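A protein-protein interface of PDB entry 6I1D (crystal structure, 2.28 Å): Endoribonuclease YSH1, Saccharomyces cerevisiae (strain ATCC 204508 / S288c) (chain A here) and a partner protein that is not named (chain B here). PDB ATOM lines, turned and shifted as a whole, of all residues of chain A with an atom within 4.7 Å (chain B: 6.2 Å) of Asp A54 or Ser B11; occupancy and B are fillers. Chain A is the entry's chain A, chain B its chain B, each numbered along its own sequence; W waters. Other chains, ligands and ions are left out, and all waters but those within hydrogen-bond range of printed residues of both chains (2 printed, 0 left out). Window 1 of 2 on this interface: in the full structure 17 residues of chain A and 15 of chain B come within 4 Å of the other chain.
Asp A54 touches six residues of chain B. Of the printed residues of chain A, Ser B11 touches Tyr A53, Asp A54, Arg A83, Thr A84 and Asn A85. Printed residues of chain A within 4 Å of Ser B77: Phe A52 (3.5 Å) and Glu A55 (3.3 Å). Of the printed residues of chain B, Phe A52 touches Arg B76 (3.5 Å) and Ser B77 (3.5 Å). Printed residues of chain B within 4 Å of Asn A85: Ser B11 and Arg B13. The nearest residue of chain B that does not touch Asp A54 is Gln B12 (4.8 Å).
The guanidinium group (NH1) of Arg B8 is in hydrogen-bond range of the backbone carbonyl oxygen (O) of Lys B10 (3.2 Å). The backbone carbonyl oxygen (O) of Gln B12 lies within hydrogen-bond range of the guanidinium group (NH1) of Arg B8. The backbone carbonyl oxygen (O) of Arg B8 lies within hydrogen-bond range of the backbone NH (N) of Val B74 (2.9 Å). The backbone carbonyl oxygen of Val B74 is in hydrogen-bond range of the backbone NH of Lys B10, 2.9 Å away.
OD1 of Asp A54 sits at hydrogen-bond distance from OG of Ser B11 (2.7 Å). NZ of Lys B75 is in salt-bridge range of OE1 of Glu A55, 3.8 Å away. The backbone carbonyl oxygen (O) of Arg A83 is in hydrogen-bond range of the backbone NH (N) of Arg B13, 3.2 Å away. The side-chain carboxylate (OD2) of Asp A54 is in hydrogen-bond range of the backbone NH (N) of Arg B76. The side-chain amide nitrogen of Gln B12 lies within hydrogen-bond range of the side-chain hydroxyl of Tyr A79 (2.7 Å).
Among the printed residues, pairs that only touch across the chains: Phe A52 with Arg B76 (3.5 Å), Phe A52 with Ser B77 (3.5 Å), Tyr A53 with Ser B11 (3.5 Å), Asp A54 with Phe B9 (3.4 Å), Asp A54 with Lys B10 (3.6 Å), Asp A54 with Val B74 (3.97 Å), Asp A54 with Lys B75 (3.4 Å), Glu A55 with Ser B77 (3.3 Å), Arg A83 with Ser B11 (3.9 Å), Arg A83 with Gln B12 (3.5 Å), Thr A84 with Ser B11 (3.3 Å), Thr A84 with Arg B13 (3.6 Å), Asn A85 with Ser B11 (3.9 Å) and Asn A85 with Arg B13 (3.3 Å).
Of the 9 printed residues of chain A, 8 touch a printed residue of chain B. Of the 10 printed residues of chain B, 9 touch a printed residue of chain A. Among the printed residues, Asp or Glu carboxylates within 4 Å of a Lys or Arg side-chain nitrogen of the other chain: Glu A55 with Lys B75.
Water W1 lies within hydrogen-bond range of O of Arg B76 (2.4 Å), OD2 of Asp A54 (3.2 Å) and N of Tyr A53 (3.4 Å). Water W2 lies within hydrogen-bond range of N of Asn A85 (2.8 Å) and O of Ser B11 (2.9 Å).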
ATOM      1  N   PHE A  52      -0.867   0.000  -9.788  1.00  0.00           N
ATOM      2  CA  PHE A  52      -0.155  -1.210 -10.201  1.00  0.00           C
ATOM      3  C   PHE A  52       0.631  -0.930 -11.486  1.00  0.00           C
ATOM      4  O   PHE A  52       0.364  -1.470 -12.563  1.00  0.00           O
ATOM      5  CB  PHE A  52      -1.128  -2.370 -10.350  1.00  0.00           C
ATOM      6  CG  PHE A  52      -1.836  -2.722  -9.071  1.00  0.00           C
ATOM      7  CD1 PHE A  52      -1.211  -3.498  -8.106  1.00  0.00           C
ATOM      8  CD2 PHE A  52      -3.122  -2.260  -8.827  1.00  0.00           C
ATOM      9  CE1 PHE A  52      -1.862  -3.818  -6.923  1.00  0.00           C
ATOM     10  CE2 PHE A  52      -3.778  -2.575  -7.647  1.00  0.00           C
ATOM     11  CZ  PHE A  52      -3.149  -3.358  -6.693  1.00  0.00           C
ATOM     12  N   TYR A  53       1.649  -0.075 -11.331  1.00  0.00           N
ATOM     13  CA  TYR A  53       2.462   0.371 -12.456  1.00  0.00           C
ATOM     14  C   TYR A  53       3.226  -0.772 -13.114  1.00  0.00           C
ATOM     15  O   TYR A  53       3.556  -0.684 -14.304  1.00  0.00           O
ATOM     16  CB  TYR A  53       3.445   1.450 -11.994  1.00  0.00           C
ATOM     17  CG  TYR A  53       2.804   2.782 -11.686  1.00  0.00           C
ATOM     18  CD1 TYR A  53       1.907   3.360 -12.574  1.00  0.00           C
ATOM     19  CD2 TYR A  53       3.099   3.465 -10.509  1.00  0.00           C
ATOM     20  CE1 TYR A  53       1.317   4.578 -12.306  1.00  0.00           C
ATOM     21  CE2 TYR A  53       2.510   4.691 -10.229  1.00  0.00           C
ATOM     22  CZ  TYR A  53       1.617   5.239 -11.134  1.00  0.00           C
ATOM     23  OH  TYR A  53       1.020   6.454 -10.876  1.00  0.00           O
ATOM     24  N   ASP A  54       3.530  -1.840 -12.370  1.00  0.00           N
ATOM     25  CA  ASP A  54       4.288  -2.949 -12.945  1.00  0.00           C
ATOM     26  C   ASP A  54       3.539  -3.638 -14.079  1.00  0.00           C
ATOM     27  O   ASP A  54       4.152  -4.396 -14.839  1.00  0.00           O
ATOM     28  CB  ASP A  54       4.627  -3.991 -11.874  1.00  0.00           C
ATOM     29  CG  ASP A  54       5.526  -3.449 -10.779  1.00  0.00           C
ATOM     30  OD1 ASP A  54       6.271  -2.477 -11.028  1.00  0.00           O
ATOM     31  OD2 ASP A  54       5.487  -4.011  -9.661  1.00  0.00           O
ATOM     32  N   GLU A  55       2.232  -3.411 -14.201  1.00  0.00           N
ATOM     33  CA  GLU A  55       1.420  -4.074 -15.211  1.00  0.00           C
ATOM     34  C   GLU A  55       1.406  -3.343 -16.549  1.00  0.00           C
ATOM     35  O   GLU A  55       0.764  -3.822 -17.489  1.00  0.00           O
ATOM     36  CB  GLU A  55      -0.016  -4.247 -14.704  1.00  0.00           C
ATOM     37  CG  GLU A  55      -0.175  -5.321 -13.637  1.00  0.00           C
ATOM     38  CD  GLU A  55       0.372  -6.670 -14.074  1.00  0.00           C
ATOM     39  OE1 GLU A  55      -0.005  -7.142 -15.168  1.00  0.00           O
ATOM     40  OE2 GLU A  55       1.182  -7.258 -13.326  1.00  0.00           O
ATOM     41  N   PHE A  56       2.100  -2.212 -16.668  1.00  0.00           N
ATOM     42  CA  PHE A  56       2.105  -1.466 -17.917  1.00  0.00           C
ATOM     43  C   PHE A  56       3.465  -0.820 -18.130  1.00  0.00           C
ATOM     44  O   PHE A  56       4.099  -0.358 -17.178  1.00  0.00           O
ATOM     45  CB  PHE A  56       1.013  -0.392 -17.933  1.00  0.00           C
ATOM     46  CG  PHE A  56       0.890   0.317 -19.245  1.00  0.00           C
ATOM     47  CD1 PHE A  56       0.492  -0.369 -20.381  1.00  0.00           C
ATOM     48  CD2 PHE A  56       1.182   1.666 -19.350  1.00  0.00           C
ATOM     49  CE1 PHE A  56       0.381   0.279 -21.598  1.00  0.00           C
ATOM     50  CE2 PHE A  56       1.074   2.321 -20.563  1.00  0.00           C
ATOM     51  CZ  PHE A  56       0.673   1.626 -21.690  1.00  0.00           C
ATOM     52  N   TYR A  79       6.625  10.182  -7.951  1.00  0.00           N
ATOM     53  CA  TYR A  79       7.205   8.857  -8.132  1.00  0.00           C
ATOM     54  C   TYR A  79       7.280   8.484  -9.607  1.00  0.00           C
ATOM     55  O   TYR A  79       8.265   7.887 -10.053  1.00  0.00           O
ATOM     56  CB  TYR A  79       6.381   7.827  -7.358  1.00  0.00           C
ATOM     57  CG  TYR A  79       6.784   6.391  -7.605  1.00  0.00           C
ATOM     58  CD1 TYR A  79       7.711   5.763  -6.782  1.00  0.00           C
ATOM     59  CD2 TYR A  79       6.234   5.660  -8.651  1.00  0.00           C
ATOM     60  CE1 TYR A  79       8.082   4.452  -6.996  1.00  0.00           C
ATOM     61  CE2 TYR A  79       6.603   4.349  -8.876  1.00  0.00           C
ATOM     62  CZ  TYR A  79       7.525   3.750  -8.044  1.00  0.00           C
ATOM     63  OH  TYR A  79       7.890   2.441  -8.256  1.00  0.00           O
ATOM     64  N   ARG A  83      11.113   7.844 -10.576  1.00  0.00           N
ATOM     65  CA  ARG A  83      11.537   6.471 -10.336  1.00  0.00           C
ATOM     66  C   ARG A  83      11.139   5.491 -11.431  1.00  0.00           C
ATOM     67  O   ARG A  83      11.519   4.317 -11.348  1.00  0.00           O
ATOM     68  CB  ARG A  83      10.981   5.975  -8.994  1.00  0.00           C
ATOM     69  CG  ARG A  83      10.938   7.044  -7.912  1.00  0.00           C
ATOM     70  CD  ARG A  83      12.133   6.941  -6.982  1.00  0.00           C
ATOM     71  NE  ARG A  83      12.609   5.565  -6.868  1.00  0.00           N
ATOM     72  CZ  ARG A  83      12.159   4.688  -5.975  1.00  0.00           C
ATOM     73  NH1 ARG A  83      12.649   3.455  -5.950  1.00  0.00           N
ATOM     74  NH2 ARG A  83      11.215   5.040  -5.112  1.00  0.00           N
ATOM     75  N   THR A  84      10.395   5.920 -12.445  1.00  0.00           N
ATOM     76  CA  THR A  84       9.890   5.026 -13.480  1.00  0.00           C
ATOM     77  C   THR A  84      10.516   5.368 -14.830  1.00  0.00           C
ATOM     78  O   THR A  84      11.254   6.346 -14.973  1.00  0.00           O
ATOM     79  CB  THR A  84       8.365   5.102 -13.570  1.00  0.00           C
ATOM     80  OG1 THR A  84       7.989   6.313 -14.239  1.00  0.00           O
ATOM     81  CG2 THR A  84       7.743   5.086 -12.180  1.00  0.00           C
ATOM     82  N   ASN A  85      10.203   4.543 -15.830  1.00  0.00           N
ATOM     83  CA  ASN A  85      10.612   4.777 -17.209  1.00  0.00           C
ATOM     84  C   ASN A  85       9.674   5.719 -17.952  1.00  0.00           C
ATOM     85  O   ASN A  85       9.702   5.751 -19.186  1.00  0.00           O
ATOM     86  CB  ASN A  85      10.714   3.452 -17.965  1.00  0.00           C
ATOM     87  CG  ASN A  85      11.837   2.574 -17.453  1.00  0.00           C
ATOM     88  OD1 ASN A  85      12.929   3.056 -17.151  1.00  0.00           O
ATOM     89  ND2 ASN A  85      11.572   1.277 -17.349  1.00  0.00           N
ATOM     90  N   ARG B   8      14.214  -6.382  -9.528  1.00  0.00           N
ATOM     91  CA  ARG B   8      13.769  -5.048  -9.902  1.00  0.00           C
ATOM     92  C   ARG B   8      12.291  -5.113 -10.247  1.00  0.00           C
ATOM     93  O   ARG B   8      11.874  -5.981 -11.019  1.00  0.00           O
ATOM     94  CB  ARG B   8      14.576  -4.510 -11.089  1.00  0.00           C
ATOM     95  CG  ARG B   8      14.066  -3.193 -11.648  1.00  0.00           C
ATOM     96  CD  ARG B   8      14.888  -2.746 -12.849  1.00  0.00           C
ATOM     97  NE  ARG B   8      14.605  -3.550 -14.034  1.00  0.00           N
ATOM     98  CZ  ARG B   8      13.574  -3.345 -14.846  1.00  0.00           C
ATOM     99  NH1 ARG B   8      12.724  -2.355 -14.606  1.00  0.00           N
ATOM    100  NH2 ARG B   8      13.394  -4.127 -15.901  1.00  0.00           N
ATOM    101  N   PHE B   9      11.501  -4.214  -9.660  1.00  0.00           N
ATOM    102  CA  PHE B   9      10.111  -4.076 -10.075  1.00  0.00           C
ATOM    103  C   PHE B   9      10.060  -3.579 -11.512  1.00  0.00           C
ATOM    104  O   PHE B   9      10.812  -2.679 -11.899  1.00  0.00           O
ATOM    105  CB  PHE B   9       9.364  -3.116  -9.147  1.00  0.00           C
ATOM    106  CG  PHE B   9       9.179  -3.645  -7.754  1.00  0.00           C
ATOM    107  CD1 PHE B   9       8.067  -4.410  -7.427  1.00  0.00           C
ATOM    108  CD2 PHE B   9      10.118  -3.381  -6.768  1.00  0.00           C
ATOM    109  CE1 PHE B   9       7.894  -4.901  -6.143  1.00  0.00           C
ATOM    110  CE2 PHE B   9       9.953  -3.870  -5.482  1.00  0.00           C
ATOM    111  CZ  PHE B   9       8.842  -4.632  -5.169  1.00  0.00           C
ATOM    112  N   LYS B  10       9.166  -4.173 -12.310  1.00  0.00           N
ATOM    113  CA  LYS B  10       9.206  -3.960 -13.755  1.00  0.00           C
ATOM    114  C   LYS B  10       9.050  -2.492 -14.131  1.00  0.00           C
ATOM    115  O   LYS B  10       9.595  -2.055 -15.151  1.00  0.00           O
ATOM    116  CB  LYS B  10       8.130  -4.797 -14.446  1.00  0.00           C
ATOM    117  CG  LYS B  10       8.311  -4.874 -15.957  1.00  0.00           C
ATOM    118  CD  LYS B  10       7.382  -5.895 -16.584  1.00  0.00           C
ATOM    119  CE  LYS B  10       7.687  -6.087 -18.062  1.00  0.00           C
ATOM    120  NZ  LYS B  10       9.105  -6.483 -18.292  1.00  0.00           N
ATOM    121  N   SER B  11       8.323  -1.715 -13.333  1.00  0.00           N
ATOM    122  CA  SER B  11       8.121  -0.303 -13.627  1.00  0.00           C
ATOM    123  C   SER B  11       9.208   0.592 -13.043  1.00  0.00           C
ATOM    124  O   SER B  11       9.159   1.811 -13.245  1.00  0.00           O
ATOM    125  CB  SER B  11       6.751   0.155 -13.115  1.00  0.00           C
ATOM    126  OG  SER B  11       6.708   0.139 -11.698  1.00  0.00           O
ATOM    127  N   GLN B  12      10.186   0.030 -12.340  1.00  0.00           N
ATOM    128  CA  GLN B  12      11.201   0.811 -11.651  1.00  0.00           C
ATOM    129  C   GLN B  12      12.528   0.753 -12.393  1.00  0.00           C
ATOM    130  O   GLN B  12      12.827  -0.216 -13.098  1.00  0.00           O
ATOM    131  CB  GLN B  12      11.394   0.314 -10.218  1.00  0.00           C
ATOM    132  CG  GLN B  12      10.280   0.720  -9.279  1.00  0.00           C
ATOM    133  CD  GLN B  12      10.642   0.515  -7.823  1.00  0.00           C
ATOM    134  OE1 GLN B  12      11.546  -0.256  -7.501  1.00  0.00           O
ATOM    135  NE2 GLN B  12       9.939   1.208  -6.936  1.00  0.00           N
ATOM    136  N   ARG B  13      13.331   1.800 -12.205  1.00  0.00           N
ATOM    137  CA  ARG B  13      14.614   1.931 -12.884  1.00  0.00           C
ATOM    138  C   ARG B  13      15.750   1.246 -12.137  1.00  0.00           C
ATOM    139  O   ARG B  13      16.608   0.616 -12.764  1.00  0.00           O
ATOM    140  CB  ARG B  13      14.950   3.410 -13.088  1.00  0.00           C
ATOM    141  CG  ARG B  13      14.277   4.032 -14.294  1.00  0.00           C
ATOM    142  CD  ARG B  13      14.899   5.369 -14.646  1.00  0.00           C
ATOM    143  NE  ARG B  13      14.587   6.390 -13.651  1.00  0.00           N
ATOM    144  CZ  ARG B  13      14.750   7.694 -13.844  1.00  0.00           C
ATOM    145  NH1 ARG B  13      14.438   8.553 -12.883  1.00  0.00           N
ATOM    146  NH2 ARG B  13      15.224   8.142 -14.999  1.00  0.00           N
ATOM    147  N   VAL B  74      10.270  -8.426 -11.040  1.00  0.00           N
ATOM    148  CA  VAL B  74       9.159  -8.568 -10.108  1.00  0.00           C
ATOM    149  C   VAL B  74       7.995  -7.714 -10.593  1.00  0.00           C
ATOM    150  O   VAL B  74       8.189  -6.575 -11.031  1.00  0.00           O
ATOM    151  CB  VAL B  74       9.562  -8.172  -8.672  1.00  0.00           C
ATOM    152  CG1 VAL B  74       8.445  -8.516  -7.695  1.00  0.00           C
ATOM    153  CG2 VAL B  74      10.856  -8.864  -8.273  1.00  0.00           C
ATOM    154  N   LYS B  75       6.785  -8.267 -10.508  1.00  0.00           N
ATOM    155  CA  LYS B  75       5.563  -7.571 -10.898  1.00  0.00           C
ATOM    156  C   LYS B  75       4.548  -7.670  -9.768  1.00  0.00           C
ATOM    157  O   LYS B  75       4.176  -8.776  -9.361  1.00  0.00           O
ATOM    158  CB  LYS B  75       4.982  -8.156 -12.188  1.00  0.00           C
ATOM    159  CG  LYS B  75       5.840  -7.914 -13.417  1.00  0.00           C
ATOM    160  CD  LYS B  75       4.985  -7.681 -14.648  1.00  0.00           C
ATOM    161  CE  LYS B  75       4.269  -8.945 -15.071  1.00  0.00           C
ATOM    162  NZ  LYS B  75       3.337  -8.690 -16.204  1.00  0.00           N
ATOM    163  N   ARG B  76       4.104  -6.521  -9.263  1.00  0.00           N
ATOM    164  CA  ARG B  76       3.036  -6.455  -8.273  1.00  0.00           C
ATOM    165  C   ARG B  76       1.731  -6.113  -8.985  1.00  0.00           C
ATOM    166  O   ARG B  76       1.602  -5.029  -9.566  1.00  0.00           O
ATOM    167  CB  ARG B  76       3.346  -5.421  -7.190  1.00  0.00           C
ATOM    168  CG  ARG B  76       2.264  -5.308  -6.122  1.00  0.00           C
ATOM    169  CD  ARG B  76       2.517  -4.138  -5.186  1.00  0.00           C
ATOM    170  NE  ARG B  76       2.439  -2.866  -5.890  1.00  0.00           N
ATOM    171  CZ  ARG B  76       1.520  -1.933  -5.666  1.00  0.00           C
ATOM    172  NH1 ARG B  76       0.590  -2.119  -4.741  1.00  0.00           N
ATOM    173  NH2 ARG B  76       1.537  -0.809  -6.366  1.00  0.00           N
ATOM    174  N   SER B  77       0.773  -7.034  -8.941  1.00  0.00           N
ATOM    175  CA  SER B  77      -0.487  -6.934  -9.658  1.00  0.00           C
ATOM    176  C   SER B  77      -1.657  -6.938  -8.677  1.00  0.00           C
ATOM    177  O   SER B  77      -1.486  -7.286  -7.503  1.00  0.00           O
ATOM    178  CB  SER B  77      -0.624  -8.097 -10.654  1.00  0.00           C
ATOM    179  OG  SER B  77      -0.593  -9.353 -10.001  1.00  0.00           O
HETATM  180  O   HOH W   1       2.564  -2.799  -9.487  1.00  0.00           O
HETATM  181  O   HOH W   2       8.349   2.508 -15.941  1.00  0.00           O
